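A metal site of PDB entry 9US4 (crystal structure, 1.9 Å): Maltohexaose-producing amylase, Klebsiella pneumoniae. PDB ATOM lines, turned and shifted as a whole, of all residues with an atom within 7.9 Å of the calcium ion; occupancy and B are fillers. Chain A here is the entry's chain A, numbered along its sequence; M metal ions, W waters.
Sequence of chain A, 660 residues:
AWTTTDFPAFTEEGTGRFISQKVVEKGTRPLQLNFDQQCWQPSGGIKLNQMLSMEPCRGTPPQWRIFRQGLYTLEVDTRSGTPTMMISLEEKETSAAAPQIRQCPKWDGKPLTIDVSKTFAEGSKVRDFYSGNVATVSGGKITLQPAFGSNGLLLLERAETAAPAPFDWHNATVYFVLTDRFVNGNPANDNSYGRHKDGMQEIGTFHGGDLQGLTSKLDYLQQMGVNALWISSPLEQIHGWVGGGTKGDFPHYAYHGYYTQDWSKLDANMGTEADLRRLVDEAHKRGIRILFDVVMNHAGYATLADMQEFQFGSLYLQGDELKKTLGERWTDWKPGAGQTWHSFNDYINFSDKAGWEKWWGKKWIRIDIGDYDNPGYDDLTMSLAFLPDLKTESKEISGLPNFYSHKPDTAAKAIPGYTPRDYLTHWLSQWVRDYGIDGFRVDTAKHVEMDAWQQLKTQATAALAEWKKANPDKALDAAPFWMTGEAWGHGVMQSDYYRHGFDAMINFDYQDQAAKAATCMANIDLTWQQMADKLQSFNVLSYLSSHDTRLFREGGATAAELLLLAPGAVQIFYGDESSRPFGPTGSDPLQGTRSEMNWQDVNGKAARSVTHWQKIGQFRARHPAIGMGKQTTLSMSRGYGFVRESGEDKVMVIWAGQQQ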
ATOM      1  N   MET A 296     -10.765 -30.608   4.953  1.00  0.00           N
ATOM      2  CA  MET A 296     -10.407 -29.221   4.571  1.00  0.00           C
ATOM      3  C   MET A 296     -10.498 -29.048   3.043  1.00  0.00           C
ATOM      4  O   MET A 296     -10.456 -27.896   2.588  1.00  0.00           O
ATOM      5  CB  MET A 296      -8.997 -28.851   5.043  1.00  0.00           C
ATOM      6  CG  MET A 296      -8.972 -28.359   6.479  1.00  0.00           C
ATOM      7  SD  MET A 296      -7.335 -27.863   7.058  1.00  0.00           S
ATOM      8  CE  MET A 296      -6.846 -26.681   5.804  1.00  0.00           C
ATOM      9  N   ASN A 297     -10.626 -30.148   2.295  1.00  0.00           N
ATOM     10  CA  ASN A 297     -10.669 -30.126   0.807  1.00  0.00           C
ATOM     11  C   ASN A 297     -11.944 -29.422   0.312  1.00  0.00           C
ATOM     12  O   ASN A 297     -11.852 -28.637  -0.654  1.00  0.00           O
ATOM     13  CB  ASN A 297     -10.621 -31.534   0.202  1.00  0.00           C
ATOM     14  CG  ASN A 297     -10.673 -31.498  -1.304  1.00  0.00           C
ATOM     15  OD1 ASN A 297      -9.771 -30.944  -1.937  1.00  0.00           O
ATOM     16  ND2 ASN A 297     -11.735 -32.034  -1.879  1.00  0.00           N
ATOM     17  N   HIS A 298     -13.087 -29.710   0.923  1.00  0.00           N
ATOM     18  CA  HIS A 298     -14.415 -29.353   0.349  1.00  0.00           C
ATOM     19  C   HIS A 298     -15.427 -29.039   1.452  1.00  0.00           C
ATOM     20  O   HIS A 298     -15.269 -29.548   2.576  1.00  0.00           O
ATOM     21  CB  HIS A 298     -14.908 -30.471  -0.567  1.00  0.00           C
ATOM     22  CG  HIS A 298     -15.067 -31.795   0.119  1.00  0.00           C
ATOM     23  ND1 HIS A 298     -14.101 -32.784   0.063  1.00  0.00           N
ATOM     24  CD2 HIS A 298     -16.079 -32.291   0.872  1.00  0.00           C
ATOM     25  CE1 HIS A 298     -14.511 -33.833   0.754  1.00  0.00           C
ATOM     26  NE2 HIS A 298     -15.715 -33.552   1.271  1.00  0.00           N
ATOM     27  N   ARG A 366     -13.719 -23.129  -5.388  1.00  0.00           N
ATOM     28  CA  ARG A 366     -13.800 -23.430  -6.835  1.00  0.00           C
ATOM     29  C   ARG A 366     -14.986 -24.383  -7.052  1.00  0.00           C
ATOM     30  O   ARG A 366     -15.102 -25.362  -6.290  1.00  0.00           O
ATOM     31  CB  ARG A 366     -12.525 -24.111  -7.361  1.00  0.00           C
ATOM     32  CG  ARG A 366     -11.314 -23.203  -7.464  1.00  0.00           C
ATOM     33  CD  ARG A 366     -10.075 -24.026  -7.772  1.00  0.00           C
ATOM     34  NE  ARG A 366      -9.614 -24.747  -6.587  1.00  0.00           N
ATOM     35  CZ  ARG A 366      -8.767 -24.267  -5.685  1.00  0.00           C
ATOM     36  NH1 ARG A 366      -8.417 -25.016  -4.653  1.00  0.00           N
ATOM     37  NH2 ARG A 366      -8.253 -23.056  -5.816  1.00  0.00           N
ATOM     38  N   ASP A 378      -6.380 -30.891 -12.070  1.00  0.00           N
ATOM     39  CA  ASP A 378      -5.387 -31.611 -11.228  1.00  0.00           C
ATOM     40  C   ASP A 378      -6.042 -31.998  -9.897  1.00  0.00           C
ATOM     41  O   ASP A 378      -7.116 -31.451  -9.591  1.00  0.00           O
ATOM     42  CB  ASP A 378      -4.137 -30.769 -10.988  1.00  0.00           C
ATOM     43  CG  ASP A 378      -4.389 -29.596 -10.053  1.00  0.00           C
ATOM     44  OD1 ASP A 378      -4.980 -28.602 -10.506  1.00  0.00           O
ATOM     45  OD2 ASP A 378      -4.015 -29.700  -8.877  1.00  0.00           O
ATOM     46  N   ASP A 379      -5.404 -32.883  -9.130  1.00  0.00           N
ATOM     47  CA  ASP A 379      -5.926 -33.415  -7.841  1.00  0.00           C
ATOM     48  C   ASP A 379      -6.185 -32.268  -6.857  1.00  0.00           C
ATOM     49  O   ASP A 379      -7.187 -32.353  -6.125  1.00  0.00           O
ATOM     50  CB  ASP A 379      -4.984 -34.449  -7.230  1.00  0.00           C
ATOM     51  CG  ASP A 379      -5.114 -35.854  -7.810  1.00  0.00           C
ATOM     52  OD1 ASP A 379      -6.210 -36.206  -8.276  1.00  0.00           O
ATOM     53  OD2 ASP A 379      -4.107 -36.584  -7.787  1.00  0.00           O
ATOM     54  N   LEU A 380      -5.332 -31.229  -6.827  1.00  0.00           N
ATOM     55  CA  LEU A 380      -5.352 -30.204  -5.744  1.00  0.00           C
ATOM     56  C   LEU A 380      -6.494 -29.197  -5.954  1.00  0.00           C
ATOM     57  O   LEU A 380      -7.058 -28.757  -4.929  1.00  0.00           O
ATOM     58  CB  LEU A 380      -3.995 -29.497  -5.657  1.00  0.00           C
ATOM     59  CG  LEU A 380      -2.822 -30.373  -5.212  1.00  0.00           C
ATOM     60  CD1 LEU A 380      -1.546 -29.558  -5.120  1.00  0.00           C
ATOM     61  CD2 LEU A 380      -3.114 -31.060  -3.884  1.00  0.00           C
ATOM     62  N   THR A 381      -6.821 -28.819  -7.197  1.00  0.00           N
ATOM     63  CA  THR A 381      -7.774 -27.707  -7.493  1.00  0.00           C
ATOM     64  C   THR A 381      -9.029 -28.215  -8.210  1.00  0.00           C
ATOM     65  O   THR A 381      -9.919 -27.383  -8.477  1.00  0.00           O
ATOM     66  CB  THR A 381      -7.087 -26.587  -8.285  1.00  0.00           C
ATOM     67  OG1 THR A 381      -6.789 -27.054  -9.604  1.00  0.00           O
ATOM     68  CG2 THR A 381      -5.809 -26.108  -7.628  1.00  0.00           C
ATOM     69  N   MET A 382      -9.132 -29.518  -8.514  1.00  0.00           N
ATOM     70  CA  MET A 382     -10.351 -30.096  -9.142  1.00  0.00           C
ATOM     71  C   MET A 382     -11.523 -30.006  -8.148  1.00  0.00           C
ATOM     72  O   MET A 382     -11.267 -29.942  -6.931  1.00  0.00           O
ATOM     73  CB  MET A 382     -10.162 -31.563  -9.547  1.00  0.00           C
ATOM     74  CG  MET A 382      -9.890 -32.499  -8.375  1.00  0.00           C
ATOM     75  SD  MET A 382      -9.702 -34.212  -8.904  1.00  0.00           S
ATOM     76  CE  MET A 382     -11.326 -34.525  -9.579  1.00  0.00           C
ATOM     77  N   SER A 383     -12.755 -30.012  -8.667  1.00  0.00           N
ATOM     78  CA  SER A 383     -14.014 -30.167  -7.906  1.00  0.00           C
ATOM     79  C   SER A 383     -14.320 -31.666  -7.802  1.00  0.00           C
ATOM     80  O   SER A 383     -14.986 -32.194  -8.703  1.00  0.00           O
ATOM     81  CB  SER A 383     -15.139 -29.396  -8.545  1.00  0.00           C
ATOM     82  OG  SER A 383     -16.355 -29.610  -7.849  1.00  0.00           O
ATOM     83  N   LEU A 384     -13.792 -32.323  -6.768  1.00  0.00           N
ATOM     84  CA  LEU A 384     -13.934 -33.790  -6.551  1.00  0.00           C
ATOM     85  C   LEU A 384     -15.415 -34.112  -6.346  1.00  0.00           C
ATOM     86  O   LEU A 384     -16.027 -33.518  -5.439  1.00  0.00           O
ATOM     87  CB  LEU A 384     -13.081 -34.194  -5.336  1.00  0.00           C
ATOM     88  CG  LEU A 384     -12.972 -35.693  -5.076  1.00  0.00           C
ATOM     89  CD1 LEU A 384     -12.273 -36.397  -6.237  1.00  0.00           C
ATOM     90  CD2 LEU A 384     -12.235 -35.944  -3.771  1.00  0.00           C
ATOM     91  N   LEU A 387     -18.009 -31.462  -5.600  1.00  0.00           N
ATOM     92  CA  LEU A 387     -17.999 -30.778  -4.282  1.00  0.00           C
ATOM     93  C   LEU A 387     -17.315 -29.420  -4.430  1.00  0.00           C
ATOM     94  O   LEU A 387     -16.332 -29.304  -5.156  1.00  0.00           O
ATOM     95  CB  LEU A 387     -17.303 -31.651  -3.234  1.00  0.00           C
ATOM     96  CG  LEU A 387     -18.031 -32.922  -2.852  1.00  0.00           C
ATOM     97  CD1 LEU A 387     -17.083 -33.953  -2.262  1.00  0.00           C
ATOM     98  CD2 LEU A 387     -19.171 -32.623  -1.888  1.00  0.00           C
ATOM     99  N   PRO A 388     -17.810 -28.361  -3.745  1.00  0.00           N
ATOM    100  CA  PRO A 388     -17.128 -27.061  -3.755  1.00  0.00           C
ATOM    101  C   PRO A 388     -15.724 -27.220  -3.170  1.00  0.00           C
ATOM    102  O   PRO A 388     -15.606 -27.668  -2.034  1.00  0.00           O
ATOM    103  CB  PRO A 388     -18.024 -26.157  -2.910  1.00  0.00           C
ATOM    104  CG  PRO A 388     -18.860 -27.103  -2.080  1.00  0.00           C
ATOM    105  CD  PRO A 388     -19.031 -28.343  -2.934  1.00  0.00           C
ATOM    106  N   ASP A 389     -14.699 -26.872  -3.951  1.00  0.00           N
ATOM    107  CA  ASP A 389     -13.275 -27.058  -3.571  1.00  0.00           C
ATOM    108  C   ASP A 389     -12.791 -25.823  -2.804  1.00  0.00           C
ATOM    109  O   ASP A 389     -12.660 -24.751  -3.435  1.00  0.00           O
ATOM    110  CB  ASP A 389     -12.409 -27.323  -4.807  1.00  0.00           C
ATOM    111  CG  ASP A 389     -11.095 -27.976  -4.456  1.00  0.00           C
ATOM    112  OD1 ASP A 389     -11.134 -29.078  -3.861  1.00  0.00           O
ATOM    113  OD2 ASP A 389     -10.032 -27.383  -4.747  1.00  0.00           O
ATOM    114  N   LEU A 390     -12.548 -25.968  -1.506  1.00  0.00           N
ATOM    115  CA  LEU A 390     -12.061 -24.866  -0.632  1.00  0.00           C
ATOM    116  C   LEU A 390     -10.677 -24.420  -1.141  1.00  0.00           C
ATOM    117  O   LEU A 390      -9.833 -25.305  -1.426  1.00  0.00           O
ATOM    118  CB  LEU A 390     -12.025 -25.340   0.824  1.00  0.00           C
ATOM    119  CG  LEU A 390     -13.396 -25.513   1.464  1.00  0.00           C
ATOM    120  CD1 LEU A 390     -13.324 -26.421   2.678  1.00  0.00           C
ATOM    121  CD2 LEU A 390     -14.004 -24.165   1.835  1.00  0.00           C
ATOM    122  N   LYS A 391     -10.486 -23.119  -1.302  1.00  0.00           N
ATOM    123  CA  LYS A 391      -9.253 -22.506  -1.880  1.00  0.00           C
ATOM    124  C   LYS A 391      -8.195 -22.448  -0.777  1.00  0.00           C
ATOM    125  O   LYS A 391      -7.863 -21.342  -0.311  1.00  0.00           O
ATOM    126  CB  LYS A 391      -9.588 -21.150  -2.507  1.00  0.00           C
ATOM    127  CG  LYS A 391     -10.422 -21.234  -3.778  1.00  0.00           C
ATOM    128  CD  LYS A 391     -11.044 -19.919  -4.217  1.00  0.00           C
ATOM    129  CE  LYS A 391     -10.041 -18.786  -4.351  1.00  0.00           C
ATOM    130  NZ  LYS A 391     -10.631 -17.620  -5.042  1.00  0.00           N
ATOM    131  N   THR A 392      -7.684 -23.621  -0.375  1.00  0.00           N
ATOM    132  CA  THR A 392      -6.715 -23.802   0.725  1.00  0.00           C
ATOM    133  C   THR A 392      -5.386 -23.110   0.388  1.00  0.00           C
ATOM    134  O   THR A 392      -4.716 -22.652   1.334  1.00  0.00           O
ATOM    135  CB  THR A 392      -6.522 -25.296   1.024  1.00  0.00           C
ATOM    136  OG1 THR A 392      -6.231 -25.957  -0.206  1.00  0.00           O
ATOM    137  CG2 THR A 392      -7.744 -25.931   1.658  1.00  0.00           C
ATOM    138  N   GLU A 393      -5.032 -23.029  -0.890  1.00  0.00           N
ATOM    139  CA  GLU A 393      -3.750 -22.444  -1.388  1.00  0.00           C
ATOM    140  C   GLU A 393      -3.854 -20.914  -1.501  1.00  0.00           C
ATOM    141  O   GLU A 393      -2.786 -20.274  -1.694  1.00  0.00           O
ATOM    142  CB  GLU A 393      -3.345 -23.061  -2.723  1.00  0.00           C
ATOM    143  CG  GLU A 393      -4.149 -22.570  -3.926  1.00  0.00           C
ATOM    144  CD  GLU A 393      -5.638 -22.842  -3.849  1.00  0.00           C
ATOM    145  OE1 GLU A 393      -6.029 -23.956  -3.440  1.00  0.00           O
ATOM    146  OE2 GLU A 393      -6.423 -21.925  -4.192  1.00  0.00           O
ATOM    147  N   THR A 444      -9.466 -36.940   2.055  1.00  0.00           N
ATOM    148  CA  THR A 444      -9.096 -36.305   0.758  1.00  0.00           C
ATOM    149  C   THR A 444      -7.699 -35.665   0.879  1.00  0.00           C
ATOM    150  O   THR A 444      -7.520 -34.523   0.399  1.00  0.00           O
ATOM    151  CB  THR A 444     -10.191 -35.345   0.304  1.00  0.00           C
ATOM    152  OG1 THR A 444     -10.826 -34.737   1.440  1.00  0.00           O
ATOM    153  CG2 THR A 444     -11.266 -36.025  -0.519  1.00  0.00           C
ATOM    154  N   LYS A 446      -4.885 -36.156  -0.640  1.00  0.00           N
ATOM    155  CA  LYS A 446      -4.162 -35.897  -1.908  1.00  0.00           C
ATOM    156  C   LYS A 446      -4.832 -34.786  -2.722  1.00  0.00           C
ATOM    157  O   LYS A 446      -4.370 -34.538  -3.847  1.00  0.00           O
ATOM    158  CB  LYS A 446      -4.010 -37.191  -2.720  1.00  0.00           C
ATOM    159  CG  LYS A 446      -5.279 -37.711  -3.373  1.00  0.00           C
ATOM    160  CD  LYS A 446      -5.082 -39.062  -4.030  1.00  0.00           C
ATOM    161  CE  LYS A 446      -4.056 -39.035  -5.144  1.00  0.00           C
ATOM    162  NZ  LYS A 446      -4.349 -40.024  -6.204  1.00  0.00           N
ATOM    163  N   HIS A 447      -5.853 -34.116  -2.181  1.00  0.00           N
ATOM    164  CA  HIS A 447      -6.628 -33.047  -2.886  1.00  0.00           C
ATOM    165  C   HIS A 447      -6.402 -31.685  -2.227  1.00  0.00           C
ATOM    166  O   HIS A 447      -7.030 -30.711  -2.687  1.00  0.00           O
ATOM    167  CB  HIS A 447      -8.104 -33.451  -2.974  1.00  0.00           C
ATOM    168  CG  HIS A 447      -8.303 -34.709  -3.744  1.00  0.00           C
ATOM    169  ND1 HIS A 447      -8.237 -34.728  -5.126  1.00  0.00           N
ATOM    170  CD2 HIS A 447      -8.490 -35.989  -3.346  1.00  0.00           C
ATOM    171  CE1 HIS A 447      -8.422 -35.966  -5.544  1.00  0.00           C
ATOM    172  NE2 HIS A 447      -8.573 -36.757  -4.476  1.00  0.00           N
ATOM    173  N   VAL A 448      -5.525 -31.605  -1.226  1.00  0.00           N
ATOM    174  CA  VAL A 448      -5.123 -30.352  -0.527  1.00  0.00           C
ATOM    175  C   VAL A 448      -3.591 -30.323  -0.461  1.00  0.00           C
ATOM    176  O   VAL A 448      -3.003 -31.383  -0.165  1.00  0.00           O
ATOM    177  CB  VAL A 448      -5.774 -30.275   0.874  1.00  0.00           C
ATOM    178  CG1 VAL A 448      -5.141 -29.196   1.740  1.00  0.00           C
ATOM    179  CG2 VAL A 448      -7.278 -30.077   0.771  1.00  0.00           C
ATOM    180  N   GLU A 449      -2.988 -29.167  -0.752  1.00  0.00           N
ATOM    181  CA  GLU A 449      -1.502 -28.993  -0.801  1.00  0.00           C
ATOM    182  C   GLU A 449      -0.905 -29.350   0.564  1.00  0.00           C
ATOM    183  O   GLU A 449      -1.596 -29.166   1.588  1.00  0.00           O
ATOM    184  CB  GLU A 449      -1.126 -27.581  -1.272  1.00  0.00           C
ATOM    185  CG  GLU A 449      -1.421 -26.469  -0.279  1.00  0.00           C
ATOM    186  CD  GLU A 449      -2.865 -25.986  -0.238  1.00  0.00           C
ATOM    187  OE1 GLU A 449      -3.699 -26.502  -1.003  1.00  0.00           O
ATOM    188  OE2 GLU A 449      -3.153 -25.079   0.566  1.00  0.00           O
HETATM  189 CA    CA M   1      -8.711 -29.208  -3.324  1.00  0.00          CA
HETATM  190  O   HOH W   1      -9.528 -27.886  -1.519  1.00  0.00           O
HETATM  191  O   HOH W   2      -9.161 -30.885  -5.168  1.00  0.00           O
HETATM  192  O   HOH W   3      -7.088 -27.459  -2.742  1.00  0.00           O
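Within 4 Å of the calcium ion: Asn 297, Leu 380, Asp 389 and His 447.
ND1 of His 447 sits at hydrogen-bond distance from O of Asp 379 (2.8 Å).
The backbone carbonyl oxygen of Asp 389 sits at hydrogen-bond distance from the backbone NH of Arg 366 (2.8 Å).
O of Asn 297 is in hydrogen-bond range of N of Leu 390.
The backbone NH (N) of Leu 380 lies within hydrogen-bond range of the side-chain carboxylate (OD2) of Asp 378 (2.9 Å).
The side-chain amide nitrogen (ND2) of Asn 297 is in hydrogen-bond range of a ring nitrogen (ND1) of His 298, at 3.2 Å.
Water W1 bridges O of Asn 297 (2.6 Å) and O of Leu 390 (2.6 Å).
Water W3 lies within hydrogen-bond range of the side-chain hydroxyl (OG1) of Thr 392 and the guanidinium group (NH1) of Arg 366.
The calcium ion is bound by O of His 447 (2.3 Å), O of Leu 380 (2.3 Å), water W1 (2.4 Å), water W3 (2.5 Å), OD1 of Asn 297 (2.5 Å), OD1 of Asp 389 (2.5 Å), water W2 (2.5 Å) and OD2 of Asp 389 (2.7 Å).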
